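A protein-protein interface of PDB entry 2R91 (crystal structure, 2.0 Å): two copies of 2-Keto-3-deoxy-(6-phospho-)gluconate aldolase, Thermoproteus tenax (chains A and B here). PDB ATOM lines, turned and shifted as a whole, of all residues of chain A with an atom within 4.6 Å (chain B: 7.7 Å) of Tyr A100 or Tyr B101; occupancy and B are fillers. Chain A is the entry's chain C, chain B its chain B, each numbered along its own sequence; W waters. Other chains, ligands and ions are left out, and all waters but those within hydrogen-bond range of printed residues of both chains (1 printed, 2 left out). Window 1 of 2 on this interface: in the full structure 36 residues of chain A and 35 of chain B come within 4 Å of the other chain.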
ATOM      1  N   THR A  41     -25.226  16.421  21.026  1.00  0.00           N
ATOM      2  CA  THR A  41     -25.899  17.698  21.286  1.00  0.00           C
ATOM      3  C   THR A  41     -27.335  17.459  21.751  1.00  0.00           C
ATOM      4  O   THR A  41     -27.776  18.064  22.736  1.00  0.00           O
ATOM      5  CB  THR A  41     -25.877  18.634  20.019  1.00  0.00           C
ATOM      6  OG1 THR A  41     -24.513  18.927  19.705  1.00  0.00           O
ATOM      7  CG2 THR A  41     -26.652  19.922  20.313  1.00  0.00           C
ATOM      8  N   PRO A  46     -22.328  18.923  26.065  1.00  0.00           N
ATOM      9  CA  PRO A  46     -21.536  19.989  26.655  1.00  0.00           C
ATOM     10  C   PRO A  46     -22.071  20.520  27.993  1.00  0.00           C
ATOM     11  O   PRO A  46     -21.329  21.201  28.693  1.00  0.00           O
ATOM     12  CB  PRO A  46     -21.579  21.089  25.567  1.00  0.00           C
ATOM     13  CG  PRO A  46     -21.657  20.266  24.263  1.00  0.00           C
ATOM     14  CD  PRO A  46     -22.738  19.255  24.685  1.00  0.00           C
ATOM     15  N   ALA A  72     -16.282  15.099  23.955  1.00  0.00           N
ATOM     16  CA  ALA A  72     -15.702  16.454  23.952  1.00  0.00           C
ATOM     17  C   ALA A  72     -15.746  17.137  25.317  1.00  0.00           C
ATOM     18  O   ALA A  72     -16.746  17.065  26.020  1.00  0.00           O
ATOM     19  CB  ALA A  72     -16.422  17.352  22.916  1.00  0.00           C
ATOM     20  N   SER A  73     -14.689  17.860  25.657  1.00  0.00           N
ATOM     21  CA  SER A  73     -14.716  18.734  26.819  1.00  0.00           C
ATOM     22  C   SER A  73     -13.797  19.909  26.538  1.00  0.00           C
ATOM     23  O   SER A  73     -12.840  19.778  25.777  1.00  0.00           O
ATOM     24  CB  SER A  73     -14.240  17.971  28.080  1.00  0.00           C
ATOM     25  OG  SER A  73     -14.048  18.854  29.193  1.00  0.00           O
ATOM     26  N   LEU A  74     -14.095  21.048  27.142  1.00  0.00           N
ATOM     27  CA  LEU A  74     -13.199  22.220  27.026  1.00  0.00           C
ATOM     28  C   LEU A  74     -12.035  22.143  28.031  1.00  0.00           C
ATOM     29  O   LEU A  74     -11.197  23.044  28.105  1.00  0.00           O
ATOM     30  CB  LEU A  74     -13.984  23.531  27.155  1.00  0.00           C
ATOM     31  CG  LEU A  74     -15.019  23.778  26.063  1.00  0.00           C
ATOM     32  CD1 LEU A  74     -15.678  25.159  26.221  1.00  0.00           C
ATOM     33  CD2 LEU A  74     -14.297  23.691  24.707  1.00  0.00           C
ATOM     34  N   LEU A  97     -16.828  16.360  19.226  1.00  0.00           N
ATOM     35  CA  LEU A  97     -16.862  17.691  18.620  1.00  0.00           C
ATOM     36  C   LEU A  97     -15.445  18.227  18.520  1.00  0.00           C
ATOM     37  O   LEU A  97     -14.577  17.873  19.342  1.00  0.00           O
ATOM     38  CB  LEU A  97     -17.652  18.619  19.514  1.00  0.00           C
ATOM     39  CG  LEU A  97     -19.130  18.288  19.761  1.00  0.00           C
ATOM     40  CD1 LEU A  97     -19.549  19.076  20.992  1.00  0.00           C
ATOM     41  CD2 LEU A  97     -19.984  18.700  18.543  1.00  0.00           C
ATOM     42  N   PRO A  98     -15.205  19.143  17.553  1.00  0.00           N
ATOM     43  CA  PRO A  98     -13.981  19.907  17.636  1.00  0.00           C
ATOM     44  C   PRO A  98     -14.101  20.803  18.845  1.00  0.00           C
ATOM     45  O   PRO A  98     -15.211  21.041  19.336  1.00  0.00           O
ATOM     46  CB  PRO A  98     -13.997  20.763  16.327  1.00  0.00           C
ATOM     47  CG  PRO A  98     -15.000  20.008  15.395  1.00  0.00           C
ATOM     48  CD  PRO A  98     -16.046  19.549  16.406  1.00  0.00           C
ATOM     49  N   PRO A  99     -12.969  21.333  19.315  1.00  0.00           N
ATOM     50  CA  PRO A  99     -12.999  22.337  20.371  1.00  0.00           C
ATOM     51  C   PRO A  99     -13.984  23.469  20.008  1.00  0.00           C
ATOM     52  O   PRO A  99     -13.941  24.029  18.889  1.00  0.00           O
ATOM     53  CB  PRO A  99     -11.560  22.841  20.400  1.00  0.00           C
ATOM     54  CG  PRO A  99     -10.733  21.662  19.940  1.00  0.00           C
ATOM     55  CD  PRO A  99     -11.592  21.037  18.836  1.00  0.00           C
ATOM     56  N   TYR A 100     -14.902  23.767  20.913  1.00  0.00           N
ATOM     57  CA  TYR A 100     -15.952  24.692  20.584  1.00  0.00           C
ATOM     58  C   TYR A 100     -15.837  25.948  21.424  1.00  0.00           C
ATOM     59  O   TYR A 100     -14.838  26.132  22.138  1.00  0.00           O
ATOM     60  CB  TYR A 100     -17.326  24.052  20.747  1.00  0.00           C
ATOM     61  CG  TYR A 100     -17.517  23.328  22.076  1.00  0.00           C
ATOM     62  CD1 TYR A 100     -18.126  23.968  23.168  1.00  0.00           C
ATOM     63  CD2 TYR A 100     -17.117  21.994  22.222  1.00  0.00           C
ATOM     64  CE1 TYR A 100     -18.322  23.269  24.407  1.00  0.00           C
ATOM     65  CE2 TYR A 100     -17.297  21.309  23.433  1.00  0.00           C
ATOM     66  CZ  TYR A 100     -17.896  21.952  24.502  1.00  0.00           C
ATOM     67  OH  TYR A 100     -18.053  21.240  25.655  1.00  0.00           O
ATOM     68  N   TYR A 101     -16.863  26.802  21.322  1.00  0.00           N
ATOM     69  CA  TYR A 101     -16.928  28.116  22.016  1.00  0.00           C
ATOM     70  C   TYR A 101     -15.864  29.140  21.580  1.00  0.00           C
ATOM     71  O   TYR A 101     -16.222  30.206  21.093  1.00  0.00           O
ATOM     72  CB  TYR A 101     -17.001  28.017  23.577  1.00  0.00           C
ATOM     73  CG  TYR A 101     -17.131  29.400  24.168  1.00  0.00           C
ATOM     74  CD1 TYR A 101     -18.372  30.020  24.232  1.00  0.00           C
ATOM     75  CD2 TYR A 101     -16.001  30.128  24.561  1.00  0.00           C
ATOM     76  CE1 TYR A 101     -18.509  31.308  24.708  1.00  0.00           C
ATOM     77  CE2 TYR A 101     -16.124  31.433  25.026  1.00  0.00           C
ATOM     78  CZ  TYR A 101     -17.387  32.004  25.085  1.00  0.00           C
ATOM     79  OH  TYR A 101     -17.538  33.282  25.511  1.00  0.00           O
ATOM     80  N   PHE A 102     -14.579  28.852  21.800  1.00  0.00           N
ATOM     81  CA  PHE A 102     -13.520  29.816  21.561  1.00  0.00           C
ATOM     82  C   PHE A 102     -13.349  30.077  20.066  1.00  0.00           C
ATOM     83  O   PHE A 102     -13.177  29.144  19.296  1.00  0.00           O
ATOM     84  CB  PHE A 102     -12.179  29.346  22.168  1.00  0.00           C
ATOM     85  CG  PHE A 102     -12.256  29.170  23.683  1.00  0.00           C
ATOM     86  CD1 PHE A 102     -12.140  30.282  24.522  1.00  0.00           C
ATOM     87  CD2 PHE A 102     -12.523  27.938  24.237  1.00  0.00           C
ATOM     88  CE1 PHE A 102     -12.242  30.154  25.896  1.00  0.00           C
ATOM     89  CE2 PHE A 102     -12.637  27.778  25.642  1.00  0.00           C
ATOM     90  CZ  PHE A 102     -12.511  28.899  26.459  1.00  0.00           C
ATOM     91  N   TYR A 130     -20.405  19.727  13.777  1.00  0.00           N
ATOM     92  CA  TYR A 130     -21.698  20.410  13.928  1.00  0.00           C
ATOM     93  C   TYR A 130     -21.377  21.914  13.887  1.00  0.00           C
ATOM     94  O   TYR A 130     -21.381  22.598  14.898  1.00  0.00           O
ATOM     95  CB  TYR A 130     -22.342  20.041  15.264  1.00  0.00           C
ATOM     96  CG  TYR A 130     -23.797  20.434  15.436  1.00  0.00           C
ATOM     97  CD1 TYR A 130     -24.587  19.835  16.429  1.00  0.00           C
ATOM     98  CD2 TYR A 130     -24.384  21.418  14.631  1.00  0.00           C
ATOM     99  CE1 TYR A 130     -25.916  20.204  16.618  1.00  0.00           C
ATOM    100  CE2 TYR A 130     -25.717  21.788  14.810  1.00  0.00           C
ATOM    101  CZ  TYR A 130     -26.468  21.183  15.807  1.00  0.00           C
ATOM    102  OH  TYR A 130     -27.797  21.542  15.946  1.00  0.00           O
ATOM    103  N   ALA A 133     -23.303  24.732  15.901  1.00  0.00           N
ATOM    104  CA  ALA A 133     -23.188  24.727  17.369  1.00  0.00           C
ATOM    105  C   ALA A 133     -21.753  25.020  17.815  1.00  0.00           C
ATOM    106  O   ALA A 133     -21.536  25.766  18.757  1.00  0.00           O
ATOM    107  CB  ALA A 133     -23.635  23.348  17.930  1.00  0.00           C
ATOM    108  N   VAL A 134     -20.788  24.409  17.120  1.00  0.00           N
ATOM    109  CA  VAL A 134     -19.365  24.470  17.463  1.00  0.00           C
ATOM    110  C   VAL A 134     -18.712  25.834  17.151  1.00  0.00           C
ATOM    111  O   VAL A 134     -17.808  26.282  17.894  1.00  0.00           O
ATOM    112  CB  VAL A 134     -18.642  23.308  16.726  1.00  0.00           C
ATOM    113  CG1 VAL A 134     -17.098  23.416  16.805  1.00  0.00           C
ATOM    114  CG2 VAL A 134     -19.178  21.947  17.253  1.00  0.00           C
ATOM    115  N   ARG A 136     -17.080  26.298  14.357  1.00  0.00           N
ATOM    116  CA  ARG A 136     -16.008  25.991  13.408  1.00  0.00           C
ATOM    117  C   ARG A 136     -16.337  24.659  12.742  1.00  0.00           C
ATOM    118  O   ARG A 136     -17.155  23.876  13.257  1.00  0.00           O
ATOM    119  CB  ARG A 136     -14.608  25.963  14.065  1.00  0.00           C
ATOM    120  CG  ARG A 136     -14.442  24.967  15.261  1.00  0.00           C
ATOM    121  CD  ARG A 136     -12.965  24.864  15.718  1.00  0.00           C
ATOM    122  NE  ARG A 136     -12.375  26.199  15.880  1.00  0.00           N
ATOM    123  CZ  ARG A 136     -12.555  27.004  16.921  1.00  0.00           C
ATOM    124  NH1 ARG A 136     -13.283  26.606  17.993  1.00  0.00           N
ATOM    125  NH2 ARG A 136     -11.989  28.200  16.894  1.00  0.00           N
ATOM    126  N   PRO B  46     -15.538  29.316  29.957  1.00  0.00           N
ATOM    127  CA  PRO B  46     -16.209  28.049  29.630  1.00  0.00           C
ATOM    128  C   PRO B  46     -15.384  26.758  29.752  1.00  0.00           C
ATOM    129  O   PRO B  46     -15.966  25.683  29.764  1.00  0.00           O
ATOM    130  CB  PRO B  46     -16.614  28.256  28.165  1.00  0.00           C
ATOM    131  CG  PRO B  46     -16.941  29.752  28.138  1.00  0.00           C
ATOM    132  CD  PRO B  46     -15.684  30.284  28.849  1.00  0.00           C
ATOM    133  N   LEU B  74     -23.118  25.776  31.506  1.00  0.00           N
ATOM    134  CA  LEU B  74     -24.204  25.045  30.847  1.00  0.00           C
ATOM    135  C   LEU B  74     -24.960  24.107  31.816  1.00  0.00           C
ATOM    136  O   LEU B  74     -25.892  23.388  31.419  1.00  0.00           O
ATOM    137  CB  LEU B  74     -23.707  24.284  29.598  1.00  0.00           C
ATOM    138  CG  LEU B  74     -23.171  25.230  28.481  1.00  0.00           C
ATOM    139  CD1 LEU B  74     -22.627  24.427  27.263  1.00  0.00           C
ATOM    140  CD2 LEU B  74     -24.214  26.230  27.995  1.00  0.00           C
ATOM    141  N   PRO B  98     -24.783  34.796  27.821  1.00  0.00           N
ATOM    142  CA  PRO B  98     -26.021  34.062  27.678  1.00  0.00           C
ATOM    143  C   PRO B  98     -25.702  32.578  27.463  1.00  0.00           C
ATOM    144  O   PRO B  98     -24.551  32.237  27.149  1.00  0.00           O
ATOM    145  CB  PRO B  98     -26.650  34.643  26.390  1.00  0.00           C
ATOM    146  CG  PRO B  98     -25.821  35.860  26.024  1.00  0.00           C
ATOM    147  CD  PRO B  98     -24.502  35.693  26.684  1.00  0.00           C
ATOM    148  N   PRO B  99     -26.707  31.693  27.647  1.00  0.00           N
ATOM    149  CA  PRO B  99     -26.511  30.279  27.343  1.00  0.00           C
ATOM    150  C   PRO B  99     -25.886  30.121  25.945  1.00  0.00           C
ATOM    151  O   PRO B  99     -26.412  30.677  24.945  1.00  0.00           O
ATOM    152  CB  PRO B  99     -27.936  29.710  27.394  1.00  0.00           C
ATOM    153  CG  PRO B  99     -28.614  30.573  28.423  1.00  0.00           C
ATOM    154  CD  PRO B  99     -28.064  31.967  28.176  1.00  0.00           C
ATOM    155  N   TYR B 100     -24.757  29.402  25.898  1.00  0.00           N
ATOM    156  CA  TYR B 100     -23.972  29.202  24.678  1.00  0.00           C
ATOM    157  C   TYR B 100     -24.022  27.755  24.167  1.00  0.00           C
ATOM    158  O   TYR B 100     -24.776  26.896  24.700  1.00  0.00           O
ATOM    159  CB  TYR B 100     -22.515  29.675  24.887  1.00  0.00           C
ATOM    160  CG  TYR B 100     -21.848  29.090  26.097  1.00  0.00           C
ATOM    161  CD1 TYR B 100     -21.050  27.945  25.994  1.00  0.00           C
ATOM    162  CD2 TYR B 100     -22.030  29.660  27.365  1.00  0.00           C
ATOM    163  CE1 TYR B 100     -20.453  27.391  27.104  1.00  0.00           C
ATOM    164  CE2 TYR B 100     -21.417  29.120  28.478  1.00  0.00           C
ATOM    165  CZ  TYR B 100     -20.635  27.980  28.336  1.00  0.00           C
ATOM    166  OH  TYR B 100     -20.036  27.464  29.470  1.00  0.00           O
ATOM    167  N   TYR B 101     -23.274  27.508  23.092  1.00  0.00           N
ATOM    168  CA  TYR B 101     -23.228  26.215  22.368  1.00  0.00           C
ATOM    169  C   TYR B 101     -24.508  25.809  21.654  1.00  0.00           C
ATOM    170  O   TYR B 101     -24.544  25.696  20.409  1.00  0.00           O
ATOM    171  CB  TYR B 101     -22.693  25.043  23.248  1.00  0.00           C
ATOM    172  CG  TYR B 101     -22.601  23.800  22.397  1.00  0.00           C
ATOM    173  CD1 TYR B 101     -21.531  23.618  21.522  1.00  0.00           C
ATOM    174  CD2 TYR B 101     -23.637  22.873  22.380  1.00  0.00           C
ATOM    175  CE1 TYR B 101     -21.467  22.513  20.688  1.00  0.00           C
ATOM    176  CE2 TYR B 101     -23.595  21.781  21.540  1.00  0.00           C
ATOM    177  CZ  TYR B 101     -22.507  21.610  20.697  1.00  0.00           C
ATOM    178  OH  TYR B 101     -22.512  20.552  19.832  1.00  0.00           O
ATOM    179  N   PHE B 102     -25.561  25.548  22.437  1.00  0.00           N
ATOM    180  CA  PHE B 102     -26.829  25.019  21.929  1.00  0.00           C
ATOM    181  C   PHE B 102     -27.532  26.004  21.024  1.00  0.00           C
ATOM    182  O   PHE B 102     -27.843  27.129  21.453  1.00  0.00           O
ATOM    183  CB  PHE B 102     -27.751  24.678  23.107  1.00  0.00           C
ATOM    184  CG  PHE B 102     -27.206  23.574  23.972  1.00  0.00           C
ATOM    185  CD1 PHE B 102     -27.284  22.245  23.542  1.00  0.00           C
ATOM    186  CD2 PHE B 102     -26.563  23.861  25.175  1.00  0.00           C
ATOM    187  CE1 PHE B 102     -26.755  21.212  24.310  1.00  0.00           C
ATOM    188  CE2 PHE B 102     -26.023  22.823  25.959  1.00  0.00           C
ATOM    189  CZ  PHE B 102     -26.129  21.493  25.520  1.00  0.00           C
ATOM    190  N   PRO B 103     -27.767  25.607  19.769  1.00  0.00           N
ATOM    191  CA  PRO B 103     -28.416  26.509  18.810  1.00  0.00           C
ATOM    192  C   PRO B 103     -29.928  26.647  19.027  1.00  0.00           C
ATOM    193  O   PRO B 103     -30.485  27.715  18.788  1.00  0.00           O
ATOM    194  CB  PRO B 103     -28.146  25.836  17.443  1.00  0.00           C
ATOM    195  CG  PRO B 103     -27.082  24.770  17.714  1.00  0.00           C
ATOM    196  CD  PRO B 103     -27.350  24.340  19.135  1.00  0.00           C
ATOM    197  N   ARG B 104     -30.594  25.602  19.482  1.00  0.00           N
ATOM    198  CA  ARG B 104     -32.057  25.614  19.434  1.00  0.00           C
ATOM    199  C   ARG B 104     -32.678  25.928  20.799  1.00  0.00           C
ATOM    200  O   ARG B 104     -33.307  25.003  21.442  1.00  0.00           O
ATOM    201  CB  ARG B 104     -32.589  24.271  18.901  1.00  0.00           C
ATOM    202  CG  ARG B 104     -31.834  23.694  17.690  1.00  0.00           C
ATOM    203  CD  ARG B 104     -32.240  24.398  16.395  1.00  0.00           C
ATOM    204  NE  ARG B 104     -31.745  23.684  15.208  1.00  0.00           N
ATOM    205  CZ  ARG B 104     -31.764  24.184  13.968  1.00  0.00           C
ATOM    206  NH1 ARG B 104     -32.245  25.412  13.733  1.00  0.00           N
ATOM    207  NH2 ARG B 104     -31.299  23.449  12.960  1.00  0.00           N
ATOM    208  N   LEU B 105     -32.444  27.179  21.264  1.00  0.00           N
ATOM    209  CA  LEU B 105     -32.928  27.620  22.570  1.00  0.00           C
ATOM    210  C   LEU B 105     -33.960  28.704  22.366  1.00  0.00           C
ATOM    211  O   LEU B 105     -33.877  29.466  21.396  1.00  0.00           O
ATOM    212  CB  LEU B 105     -31.815  28.094  23.512  1.00  0.00           C
ATOM    213  CG  LEU B 105     -30.704  27.126  24.016  1.00  0.00           C
ATOM    214  CD1 LEU B 105     -29.919  27.773  25.105  1.00  0.00           C
ATOM    215  CD2 LEU B 105     -31.206  25.740  24.492  1.00  0.00           C
ATOM    216  N   ALA B 133     -18.580  34.123  19.904  1.00  0.00           N
ATOM    217  CA  ALA B 133     -18.235  32.936  20.703  1.00  0.00           C
ATOM    218  C   ALA B 133     -19.521  32.227  21.183  1.00  0.00           C
ATOM    219  O   ALA B 133     -19.643  30.995  21.097  1.00  0.00           O
ATOM    220  CB  ALA B 133     -17.335  33.332  21.875  1.00  0.00           C
ATOM    221  N   VAL B 134     -20.502  33.010  21.636  1.00  0.00           N
ATOM    222  CA  VAL B 134     -21.746  32.442  22.201  1.00  0.00           C
ATOM    223  C   VAL B 134     -22.639  31.790  21.140  1.00  0.00           C
ATOM    224  O   VAL B 134     -23.317  30.817  21.415  1.00  0.00           O
ATOM    225  CB  VAL B 134     -22.527  33.527  22.958  1.00  0.00           C
ATOM    226  CG1 VAL B 134     -23.929  33.052  23.360  1.00  0.00           C
ATOM    227  CG2 VAL B 134     -21.709  34.019  24.159  1.00  0.00           C
ATOM    228  N   GLY B 135     -22.644  32.321  19.924  1.00  0.00           N
ATOM    229  CA  GLY B 135     -23.546  31.785  18.894  1.00  0.00           C
ATOM    230  C   GLY B 135     -24.933  32.423  18.907  1.00  0.00           C
ATOM    231  O   GLY B 135     -25.812  32.055  18.127  1.00  0.00           O
ATOM    232  N   ARG B 136     -25.143  33.374  19.800  1.00  0.00           N
ATOM    233  CA  ARG B 136     -26.387  34.126  19.819  1.00  0.00           C
ATOM    234  C   ARG B 136     -26.077  35.508  20.376  1.00  0.00           C
ATOM    235  O   ARG B 136     -25.078  35.699  21.043  1.00  0.00           O
ATOM    236  CB  ARG B 136     -27.503  33.461  20.664  1.00  0.00           C
ATOM    237  CG  ARG B 136     -28.831  34.281  20.525  1.00  0.00           C
ATOM    238  CD  ARG B 136     -30.105  33.908  21.419  1.00  0.00           C
ATOM    239  NE  ARG B 136     -30.918  32.841  20.827  1.00  0.00           N
ATOM    240  CZ  ARG B 136     -30.612  31.532  20.911  1.00  0.00           C
ATOM    241  NH1 ARG B 136     -29.488  31.106  21.602  1.00  0.00           N
ATOM    242  NH2 ARG B 136     -31.448  30.636  20.314  1.00  0.00           N
ATOM    243  N   PRO B 261      -8.098  22.364  25.188  1.00  0.00           N
ATOM    244  CA  PRO B 261      -7.762  22.320  23.758  1.00  0.00           C
ATOM    245  C   PRO B 261      -7.158  23.734  23.442  1.00  0.00           C
ATOM    246  O   PRO B 261      -6.701  23.976  22.324  1.00  0.00           O
ATOM    247  CB  PRO B 261      -9.111  22.126  23.035  1.00  0.00           C
ATOM    248  CG  PRO B 261     -10.162  22.679  24.017  1.00  0.00           C
ATOM    249  CD  PRO B 261      -9.549  22.552  25.425  1.00  0.00           C
ATOM    250  N   VAL B 262      -7.162  24.669  24.411  1.00  0.00           N
ATOM    251  CA  VAL B 262      -6.372  25.913  24.262  1.00  0.00           C
ATOM    252  C   VAL B 262      -4.922  25.645  24.652  1.00  0.00           C
ATOM    253  O   VAL B 262      -4.468  26.083  25.732  1.00  0.00           O
ATOM    254  CB  VAL B 262      -6.937  27.120  25.051  1.00  0.00           C
ATOM    255  CG1 VAL B 262      -6.239  28.435  24.595  1.00  0.00           C
ATOM    256  CG2 VAL B 262      -8.515  27.214  24.867  1.00  0.00           C
HETATM  257  O   HOH W   1     -28.789  23.398  14.222  1.00  0.00           O
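The side-chain hydroxyl (OG1) of Thr A41 lies within hydrogen-bond range of the side-chain hydroxyl (OH) of Tyr B101 (2.6 Å).
O of Ala A133 sits close to O of Tyr B101 (3.4 Å).
The backbone carbonyl oxygen (O) of Pro B103 lies within hydrogen-bond range of the guanidinium group (NH2) of Arg B136, at 3.4 Å.
The backbone carbonyl oxygen (O) of Pro A99 is in hydrogen-bond range of the guanidinium group (NH1) of Arg A136 (2.8 Å).
CE1 of Phe B102 touches O of Thr A41, at 3.7 Å.
Tyr B101 touches Pro A46.
O of Pro B46 touches CD1 of Leu A74, 3.6 Å away.
Pro B261 touches Leu A74 (CD to O, 3.2 Å).
CG of Pro A99 touches CB of Pro B261, 3.5 Å away.
Tyr B101 touches Tyr A100 (CD1 to CD1, 3.8 Å).
Tyr B100 touches Tyr A101 (CD1 to CD1, 3.8 Å).
O of Tyr A101 touches CB of Ala B133 (3.4 Å).
Tyr A130 touches Pro B103 (OH to CG, 3.7 Å).
Ala A133 touches Pro B103 (CB to CG, 3.7 Å).
Of chain B, only Tyr B101 comes within 4 Å of Tyr A100.
Val A134 touches none of the printed residues of chain B.
Tyr B101 touches five residues of chain A.
Of the printed residues of chain A, Phe B102 touches Thr A41.
Of the printed residues of chain A, Ala B133 touches Tyr A101 (3.4 Å).
Val B134 touches none of the printed residues of chain A.
The nearest residue of chain B that does not touch Tyr A100 is Leu B74 (5.3 Å).
The nearest printed residue of chain B that does not touch Leu A97 is Pro B261 (7.8 Å).
Along chain B the printed residues that touch a printed residue of chain A span positions 46 to 261.
Printed residues of chain A that touch a printed residue of chain B: Thr A41, Pro A46, Leu A74, Leu A97, Pro A99, Tyr A100, Tyr A101, Tyr A130 and Ala A133.
Hydrophobic or aromatic side chains of chain A that line the printed part of chain B: Pro A46, Leu A74, Leu A97, Pro A99, Tyr A100, Tyr A101, Tyr A130 and Ala A133.
Among the printed residues, no Asp or Glu carboxylate lies within 4 Å of a Lys or Arg side-chain nitrogen of the other chain.
Pro A46 touches Leu B74, and with the chains exchanged Leu A74 touches Pro B46.
Pro A46 touches Tyr B101, and with the chains exchanged Tyr A101 touches Pro B46.
Tyr A100 touches Tyr B101, and with the chains exchanged Tyr A101 touches Tyr B100.
Tyr A101 touches Ala B133, and with the chains exchanged Ala A133 touches Tyr B101.
Positions printed for both chains: 46, 74, 98, 99, 100, 101, 102, 133, 134 and 136.
Water W1 bridges OH of Tyr A130 (2.7 Å) and NH2 of Arg B104 (2.8 Å).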
